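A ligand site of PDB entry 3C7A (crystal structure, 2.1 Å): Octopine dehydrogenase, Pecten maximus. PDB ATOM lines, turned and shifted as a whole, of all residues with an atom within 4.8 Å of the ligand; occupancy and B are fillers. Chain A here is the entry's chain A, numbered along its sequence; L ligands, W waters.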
ATOM      1  N   GLY A   9       6.404  21.874   3.659  1.00  0.00           N
ATOM      2  CA  GLY A   9       4.966  22.092   3.918  1.00  0.00           C
ATOM      3  C   GLY A   9       4.066  20.880   3.740  1.00  0.00           C
ATOM      4  O   GLY A   9       4.540  19.798   3.365  1.00  0.00           O
ATOM      5  N   GLY A  10       2.772  21.044   4.005  1.00  0.00           N
ATOM      6  CA  GLY A  10       1.799  19.951   3.883  1.00  0.00           C
ATOM      7  C   GLY A  10       0.350  20.295   3.558  1.00  0.00           C
ATOM      8  O   GLY A  10      -0.559  19.525   3.903  1.00  0.00           O
ATOM      9  N   GLY A  11       0.128  21.424   2.884  1.00  0.00           N
ATOM     10  CA  GLY A  11      -1.235  21.859   2.531  1.00  0.00           C
ATOM     11  C   GLY A  11      -1.615  21.626   1.076  1.00  0.00           C
ATOM     12  O   GLY A  11      -1.110  20.708   0.434  1.00  0.00           O
ATOM     13  N   ASN A  12      -2.517  22.474   0.554  1.00  0.00           N
ATOM     14  CA  ASN A  12      -2.993  22.374  -0.829  1.00  0.00           C
ATOM     15  C   ASN A  12      -1.855  22.495  -1.861  1.00  0.00           C
ATOM     16  O   ASN A  12      -1.792  21.712  -2.820  1.00  0.00           O
ATOM     17  CB  ASN A  12      -4.061  23.445  -1.140  1.00  0.00           C
ATOM     18  CG  ASN A  12      -5.333  23.270  -0.313  1.00  0.00           C
ATOM     19  OD1 ASN A  12      -5.885  22.169  -0.189  1.00  0.00           O
ATOM     20  ND2 ASN A  12      -5.823  24.372   0.236  1.00  0.00           N
ATOM     21  N   GLY A  13      -0.969  23.469  -1.640  1.00  0.00           N
ATOM     22  CA  GLY A  13       0.162  23.720  -2.536  1.00  0.00           C
ATOM     23  C   GLY A  13       1.242  22.655  -2.511  1.00  0.00           C
ATOM     24  O   GLY A  13       1.788  22.289  -3.556  1.00  0.00           O
ATOM     25  N   ALA A  14       1.534  22.135  -1.312  1.00  0.00           N
ATOM     26  CA  ALA A  14       2.575  21.114  -1.128  1.00  0.00           C
ATOM     27  C   ALA A  14       2.203  19.758  -1.729  1.00  0.00           C
ATOM     28  O   ALA A  14       3.077  19.033  -2.232  1.00  0.00           O
ATOM     29  CB  ALA A  14       2.936  20.976   0.344  1.00  0.00           C
ATOM     30  N   THR A  33       7.991  18.450   6.854  1.00  0.00           N
ATOM     31  CA  THR A  33       6.955  19.217   7.563  1.00  0.00           C
ATOM     32  C   THR A  33       7.180  19.224   9.085  1.00  0.00           C
ATOM     33  O   THR A  33       7.484  18.180   9.670  1.00  0.00           O
ATOM     34  CB  THR A  33       5.500  18.767   7.217  1.00  0.00           C
ATOM     35  OG1 THR A  33       4.567  19.382   8.111  1.00  0.00           O
ATOM     36  CG2 THR A  33       5.344  17.251   7.296  1.00  0.00           C
ATOM     37  N   PHE A  35       4.884  20.586  11.500  1.00  0.00           N
ATOM     38  CA  PHE A  35       3.647  20.802  12.257  1.00  0.00           C
ATOM     39  C   PHE A  35       3.253  19.566  13.067  1.00  0.00           C
ATOM     40  O   PHE A  35       2.563  18.674  12.571  1.00  0.00           O
ATOM     41  CB  PHE A  35       2.514  21.245  11.305  1.00  0.00           C
ATOM     42  CG  PHE A  35       1.219  21.603  11.998  1.00  0.00           C
ATOM     43  CD1 PHE A  35       1.209  22.347  13.173  1.00  0.00           C
ATOM     44  CD2 PHE A  35      -0.007  21.213  11.446  1.00  0.00           C
ATOM     45  CE1 PHE A  35       0.005  22.675  13.808  1.00  0.00           C
ATOM     46  CE2 PHE A  35      -1.208  21.546  12.057  1.00  0.00           C
ATOM     47  CZ  PHE A  35      -1.206  22.275  13.244  1.00  0.00           C
ATOM     48  N   GLU A  38       2.669  15.621  11.724  1.00  0.00           N
ATOM     49  CA  GLU A  38       1.999  15.607  10.414  1.00  0.00           C
ATOM     50  C   GLU A  38       2.636  14.616   9.418  1.00  0.00           C
ATOM     51  O   GLU A  38       1.937  14.046   8.575  1.00  0.00           O
ATOM     52  CB  GLU A  38       1.944  17.023   9.813  1.00  0.00           C
ATOM     53  CG  GLU A  38       0.875  17.226   8.736  1.00  0.00           C
ATOM     54  CD  GLU A  38       0.754  18.674   8.258  1.00  0.00           C
ATOM     55  OE1 GLU A  38       1.799  19.294   7.955  1.00  0.00           O
ATOM     56  OE2 GLU A  38      -0.376  19.177   8.161  1.00  0.00           O
ATOM     57  N   THR A  89       6.462  26.417   0.392  1.00  0.00           N
ATOM     58  CA  THR A  89       5.071  26.668  -0.044  1.00  0.00           C
ATOM     59  C   THR A  89       4.049  26.530   1.102  1.00  0.00           C
ATOM     60  O   THR A  89       3.379  25.502   1.247  1.00  0.00           O
ATOM     61  CB  THR A  89       4.693  25.818  -1.316  1.00  0.00           C
ATOM     62  OG1 THR A  89       3.330  26.057  -1.671  1.00  0.00           O
ATOM     63  CG2 THR A  89       4.926  24.319  -1.085  1.00  0.00           C
ATOM     64  N   VAL A  90       3.943  27.594   1.904  1.00  0.00           N
ATOM     65  CA  VAL A  90       3.121  27.637   3.127  1.00  0.00           C
ATOM     66  C   VAL A  90       2.669  29.083   3.438  1.00  0.00           C
ATOM     67  O   VAL A  90       3.189  30.021   2.838  1.00  0.00           O
ATOM     68  CB  VAL A  90       3.889  27.101   4.376  1.00  0.00           C
ATOM     69  CG1 VAL A  90       3.841  25.587   4.451  1.00  0.00           C
ATOM     70  CG2 VAL A  90       5.337  27.616   4.412  1.00  0.00           C
ATOM     71  N   PRO A  91       1.697  29.254   4.367  1.00  0.00           N
ATOM     72  CA  PRO A  91       1.421  30.598   4.909  1.00  0.00           C
ATOM     73  C   PRO A  91       2.651  31.241   5.558  1.00  0.00           C
ATOM     74  O   PRO A  91       3.493  30.546   6.122  1.00  0.00           O
ATOM     75  CB  PRO A  91       0.337  30.326   5.969  1.00  0.00           C
ATOM     76  CG  PRO A  91      -0.312  29.071   5.528  1.00  0.00           C
ATOM     77  CD  PRO A  91       0.789  28.239   4.939  1.00  0.00           C
ATOM     78  N   PHE A  93       3.499  33.028   8.208  1.00  0.00           N
ATOM     79  CA  PHE A  93       3.872  32.978   9.635  1.00  0.00           C
ATOM     80  C   PHE A  93       4.709  31.738  10.011  1.00  0.00           C
ATOM     81  O   PHE A  93       5.280  31.677  11.104  1.00  0.00           O
ATOM     82  CB  PHE A  93       2.633  33.108  10.548  1.00  0.00           C
ATOM     83  CG  PHE A  93       1.690  31.930  10.492  1.00  0.00           C
ATOM     84  CD1 PHE A  93       0.578  31.948   9.665  1.00  0.00           C
ATOM     85  CD2 PHE A  93       1.908  30.807  11.296  1.00  0.00           C
ATOM     86  CE1 PHE A  93      -0.307  30.869   9.622  1.00  0.00           C
ATOM     87  CE2 PHE A  93       1.033  29.719  11.256  1.00  0.00           C
ATOM     88  CZ  PHE A  93      -0.072  29.749  10.411  1.00  0.00           C
ATOM     89  N   ALA A  94       4.782  30.770   9.098  1.00  0.00           N
ATOM     90  CA  ALA A  94       5.510  29.522   9.334  1.00  0.00           C
ATOM     91  C   ALA A  94       6.938  29.513   8.762  1.00  0.00           C
ATOM     92  O   ALA A  94       7.666  28.526   8.938  1.00  0.00           O
ATOM     93  CB  ALA A  94       4.710  28.337   8.805  1.00  0.00           C
ATOM     94  N   PRO A 116       4.435  31.221  -2.706  1.00  0.00           N
ATOM     95  CA  PRO A 116       4.918  32.597  -2.879  1.00  0.00           C
ATOM     96  C   PRO A 116       5.690  33.140  -1.661  1.00  0.00           C
ATOM     97  O   PRO A 116       5.537  32.633  -0.548  1.00  0.00           O
ATOM     98  CB  PRO A 116       3.629  33.385  -3.096  1.00  0.00           C
ATOM     99  CG  PRO A 116       2.591  32.631  -2.299  1.00  0.00           C
ATOM    100  CD  PRO A 116       3.073  31.212  -2.122  1.00  0.00           C
ATOM    101  N   GLN A 118       5.731  36.452  -0.408  1.00  0.00           N
ATOM    102  CA  GLN A 118       5.240  37.640   0.290  1.00  0.00           C
ATOM    103  C   GLN A 118       6.399  38.661   0.683  1.00  0.00           C
ATOM    104  O   GLN A 118       7.451  38.579   0.222  1.00  0.00           O
ATOM    105  CB  GLN A 118       4.277  37.303   1.502  1.00  0.00           C
ATOM    106  CG  GLN A 118       2.905  36.666   1.105  1.00  0.00           C
ATOM    107  CD  GLN A 118       1.968  36.348   2.261  1.00  0.00           C
ATOM    108  OE1 GLN A 118       2.156  35.392   2.950  1.00  0.00           O
ATOM    109  NE2 GLN A 118       0.965  37.175   2.455  1.00  0.00           N
ATOM    110  N   THR A 143       2.877  34.993  -7.015  1.00  0.00           N
ATOM    111  CA  THR A 143       1.719  34.285  -6.415  1.00  0.00           C
ATOM    112  C   THR A 143       1.808  32.763  -6.689  1.00  0.00           C
ATOM    113  O   THR A 143       2.775  32.300  -7.296  1.00  0.00           O
ATOM    114  CB  THR A 143       0.344  34.883  -6.890  1.00  0.00           C
ATOM    115  OG1 THR A 143      -0.718  34.365  -6.089  1.00  0.00           O
ATOM    116  CG2 THR A 143       0.075  34.593  -8.364  1.00  0.00           C
ATOM    117  N   LEU A 144       0.814  31.998  -6.227  1.00  0.00           N
ATOM    118  CA  LEU A 144       0.768  30.547  -6.466  1.00  0.00           C
ATOM    119  C   LEU A 144       0.360  30.226  -7.916  1.00  0.00           C
ATOM    120  O   LEU A 144      -0.560  30.852  -8.447  1.00  0.00           O
ATOM    121  CB  LEU A 144      -0.178  29.854  -5.464  1.00  0.00           C
ATOM    122  CG  LEU A 144      -0.126  28.329  -5.321  1.00  0.00           C
ATOM    123  CD1 LEU A 144       1.123  27.870  -4.542  1.00  0.00           C
ATOM    124  CD2 LEU A 144      -1.381  27.790  -4.642  1.00  0.00           C
ATOM    125  N   TRP A 146      -1.258  27.672  -9.265  1.00  0.00           N
ATOM    126  CA  TRP A 146      -2.547  27.016  -9.488  1.00  0.00           C
ATOM    127  C   TRP A 146      -3.634  27.445  -8.492  1.00  0.00           C
ATOM    128  O   TRP A 146      -3.338  27.972  -7.422  1.00  0.00           O
ATOM    129  CB  TRP A 146      -2.410  25.477  -9.401  1.00  0.00           C
ATOM    130  CG  TRP A 146      -1.113  24.892  -9.906  1.00  0.00           C
ATOM    131  CD1 TRP A 146      -0.824  24.534 -11.201  1.00  0.00           C
ATOM    132  CD2 TRP A 146       0.045  24.565  -9.126  1.00  0.00           C
ATOM    133  NE1 TRP A 146       0.449  24.017 -11.265  1.00  0.00           N
ATOM    134  CE2 TRP A 146       1.007  24.031 -10.018  1.00  0.00           C
ATOM    135  CE3 TRP A 146       0.362  24.690  -7.773  1.00  0.00           C
ATOM    136  CZ2 TRP A 146       2.274  23.608  -9.582  1.00  0.00           C
ATOM    137  CZ3 TRP A 146       1.628  24.274  -7.344  1.00  0.00           C
ATOM    138  CH2 TRP A 146       2.563  23.736  -8.248  1.00  0.00           C
ATOM    139  N   ALA A 147      -4.892  27.194  -8.867  1.00  0.00           N
ATOM    140  CA  ALA A 147      -6.008  27.170  -7.915  1.00  0.00           C
ATOM    141  C   ALA A 147      -6.332  25.705  -7.620  1.00  0.00           C
ATOM    142  O   ALA A 147      -6.721  24.965  -8.526  1.00  0.00           O
ATOM    143  CB  ALA A 147      -7.215  27.894  -8.481  1.00  0.00           C
ATOM    144  N   CYS A 148      -6.157  25.298  -6.364  1.00  0.00           N
ATOM    145  CA  CYS A 148      -6.184  23.866  -5.995  1.00  0.00           C
ATOM    146  C   CYS A 148      -6.800  23.570  -4.615  1.00  0.00           C
ATOM    147  O   CYS A 148      -6.767  24.415  -3.725  1.00  0.00           O
ATOM    148  CB  CYS A 148      -4.765  23.270  -6.092  1.00  0.00           C
ATOM    149  SG  CYS A 148      -3.479  24.190  -5.168  1.00  0.00           S
ATOM    150  N   ARG A 324      -8.123  36.017   7.762  1.00  0.00           N
ATOM    151  CA  ARG A 324      -6.743  36.259   7.376  1.00  0.00           C
ATOM    152  C   ARG A 324      -6.514  37.441   6.450  1.00  0.00           C
ATOM    153  O   ARG A 324      -5.383  37.771   6.137  1.00  0.00           O
ATOM    154  CB  ARG A 324      -6.091  34.978   6.838  1.00  0.00           C
ATOM    155  CG  ARG A 324      -5.788  33.914   7.888  1.00  0.00           C
ATOM    156  CD  ARG A 324      -5.070  32.707   7.337  1.00  0.00           C
ATOM    157  NE  ARG A 324      -4.803  31.696   8.346  1.00  0.00           N
ATOM    158  CZ  ARG A 324      -4.403  30.464   8.064  1.00  0.00           C
ATOM    159  NH1 ARG A 324      -4.207  29.574   8.991  1.00  0.00           N
ATOM    160  NH2 ARG A 324      -4.211  30.135   6.814  1.00  0.00           N
HETATM  161  P1  LIG L   1      -2.802  25.856   3.337  1.00  0.00           P
HETATM  162  O1  LIG L   1      -3.775  26.575   4.183  1.00  0.00           O
HETATM  163  O2  LIG L   1      -3.437  24.725   2.636  1.00  0.00           O
HETATM  164  O3  LIG L   1      -1.555  25.350   4.223  1.00  0.00           O
HETATM  165  C1  LIG L   1      -1.739  24.581   5.402  1.00  0.00           C
HETATM  166  C2  LIG L   1      -0.397  24.026   5.881  1.00  0.00           C
HETATM  167  O4  LIG L   1       0.334  25.015   6.571  1.00  0.00           O
HETATM  168  C3  LIG L   1      -0.549  22.863   6.852  1.00  0.00           C
HETATM  169  O5  LIG L   1      -0.536  21.613   6.198  1.00  0.00           O
HETATM  170  C4  LIG L   1       0.630  23.010   7.793  1.00  0.00           C
HETATM  171  O6  LIG L   1       1.743  22.276   7.348  1.00  0.00           O
HETATM  172  C5  LIG L   1       0.946  24.500   7.743  1.00  0.00           C
HETATM  173  N1  LIG L   1       0.380  25.124   8.964  1.00  0.00           N
HETATM  174  C6  LIG L   1      -0.895  25.618   9.091  1.00  0.00           C
HETATM  175  N2  LIG L   1      -1.049  26.101  10.353  1.00  0.00           N
HETATM  176  C7  LIG L   1       0.106  25.908  11.023  1.00  0.00           C
HETATM  177  C8  LIG L   1       0.481  26.221  12.334  1.00  0.00           C
HETATM  178  N3  LIG L   1      -0.450  26.561  13.219  1.00  0.00           N
HETATM  179  N4  LIG L   1       1.759  25.910  12.763  1.00  0.00           N
HETATM  180  C9  LIG L   1       2.658  25.289  11.898  1.00  0.00           C
HETATM  181  N5  LIG L   1       2.273  24.995  10.606  1.00  0.00           N
HETATM  182  C10 LIG L   1       1.013  25.301  10.170  1.00  0.00           C
HETATM  183  O7  LIG L   1      -2.141  26.913   2.299  1.00  0.00           O
HETATM  184  P2  LIG L   1      -2.170  26.704   0.691  1.00  0.00           P
HETATM  185  O8  LIG L   1      -3.574  26.596   0.254  1.00  0.00           O
HETATM  186  O9  LIG L   1      -1.208  25.630   0.330  1.00  0.00           O
HETATM  187  O10 LIG L   1      -1.611  28.106   0.101  1.00  0.00           O
HETATM  188  C11 LIG L   1      -0.344  28.632   0.428  1.00  0.00           C
HETATM  189  C12 LIG L   1      -0.307  30.131   0.106  1.00  0.00           C
HETATM  190  O11 LIG L   1      -0.677  30.375  -1.252  1.00  0.00           O
HETATM  191  C13 LIG L   1      -1.274  30.917   0.986  1.00  0.00           C
HETATM  192  O12 LIG L   1      -0.615  32.060   1.487  1.00  0.00           O
HETATM  193  C14 LIG L   1      -2.408  31.312   0.058  1.00  0.00           C
HETATM  194  O13 LIG L   1      -2.936  32.572   0.389  1.00  0.00           O
HETATM  195  C15 LIG L   1      -1.748  31.304  -1.322  1.00  0.00           C
HETATM  196  N6  LIG L   1      -2.678  30.995  -2.432  1.00  0.00           N
HETATM  197  C16 LIG L   1      -3.456  29.852  -2.416  1.00  0.00           C
HETATM  198  C17 LIG L   1      -4.330  29.573  -3.480  1.00  0.00           C
HETATM  199  C18 LIG L   1      -4.989  28.224  -3.581  1.00  0.00           C
HETATM  200  O14 LIG L   1      -5.878  27.994  -4.542  1.00  0.00           O
HETATM  201  N7  LIG L   1      -4.649  27.206  -2.661  1.00  0.00           N
HETATM  202  C19 LIG L   1      -4.406  30.464  -4.553  1.00  0.00           C
HETATM  203  C20 LIG L   1      -3.615  31.613  -4.566  1.00  0.00           C
HETATM  204  C21 LIG L   1      -2.755  31.859  -3.488  1.00  0.00           C
HETATM  205  O   HOH W   1       4.747  23.922   9.116  1.00  0.00           O
HETATM  206  O   HOH W   2      -5.526  28.725   0.798  1.00  0.00           O
HETATM  207  O   HOH W   3      -1.671  33.697   3.532  1.00  0.00           O
HETATM  208  O   HOH W   4      -8.155  29.604  -5.178  1.00  0.00           O
HETATM  209  O   HOH W   5       0.906  23.905   1.261  1.00  0.00           O
HETATM  210  O   HOH W   6      -4.440  29.523   3.519  1.00  0.00           O
HETATM  211  O   HOH W   7      -1.578  35.258  -0.722  1.00  0.00           O
HETATM  212  O   HOH W   8      -3.742  26.907   7.213  1.00  0.00           O
HETATM  213  O   HOH W   9      -5.336  23.115   3.952  1.00  0.00           O
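The backbone NH (N) of Asn 12 is in hydrogen-bond range of an oxygen (O2) of the ligand (3.2 Å).
An oxygen (O5) of the ligand lies close to the backbone carbonyl oxygen (O) of Gly 10 (3.1 Å).
OE1 of Glu 38 is in hydrogen-bond range of O6 of the ligand (3.0 Å).
The backbone NH (N) of Cys 148 is in hydrogen-bond range of an oxygen (O14) of the ligand (3.3 Å).
An oxygen (O8) of the ligand lies within hydrogen-bond range of the side-chain amide nitrogen of Asn 12 (3.2 Å).
An oxygen (O9) of the ligand is in hydrogen-bond range of the backbone NH of Gly 13 (2.9 Å).
The backbone NH (N) of Gly 11 lies within hydrogen-bond range of an oxygen (O5) of the ligand, 3.4 Å away.
The side-chain carboxylate of Glu 38 lies within hydrogen-bond range of the side-chain hydroxyl of Thr 33, 2.8 Å away.
Phe 35 touches the ligand (CD1 to C9, 3.5 Å).
CD of Pro 91 touches O4 of the ligand, 3.6 Å away.
Phe 93 touches the ligand.
Pro 116 touches the ligand.
Leu 144 touches the ligand.
Trp 146 touches the ligand (O to O14, 3.8 Å).
CA of Ala 147 touches O14 of the ligand, at 3.5 Å.
Hydrophobic or aromatic side chains within 4 Å of the ligand: Phe 35, Pro 91, Phe 93, Pro 116 and Leu 144.
Of the 22 residues printed, 13 come within 4 Å of the ligand.
The nearest printed residue that does not touch the ligand is Thr 33 (4.1 Å).
Water W8 lies within hydrogen-bond range of O1 of the ligand (3.0 Å) and NH1 of Arg 324 (3.2 Å).
Water W6 lies within hydrogen-bond range of O1 of the ligand and NH2 of Arg 324.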
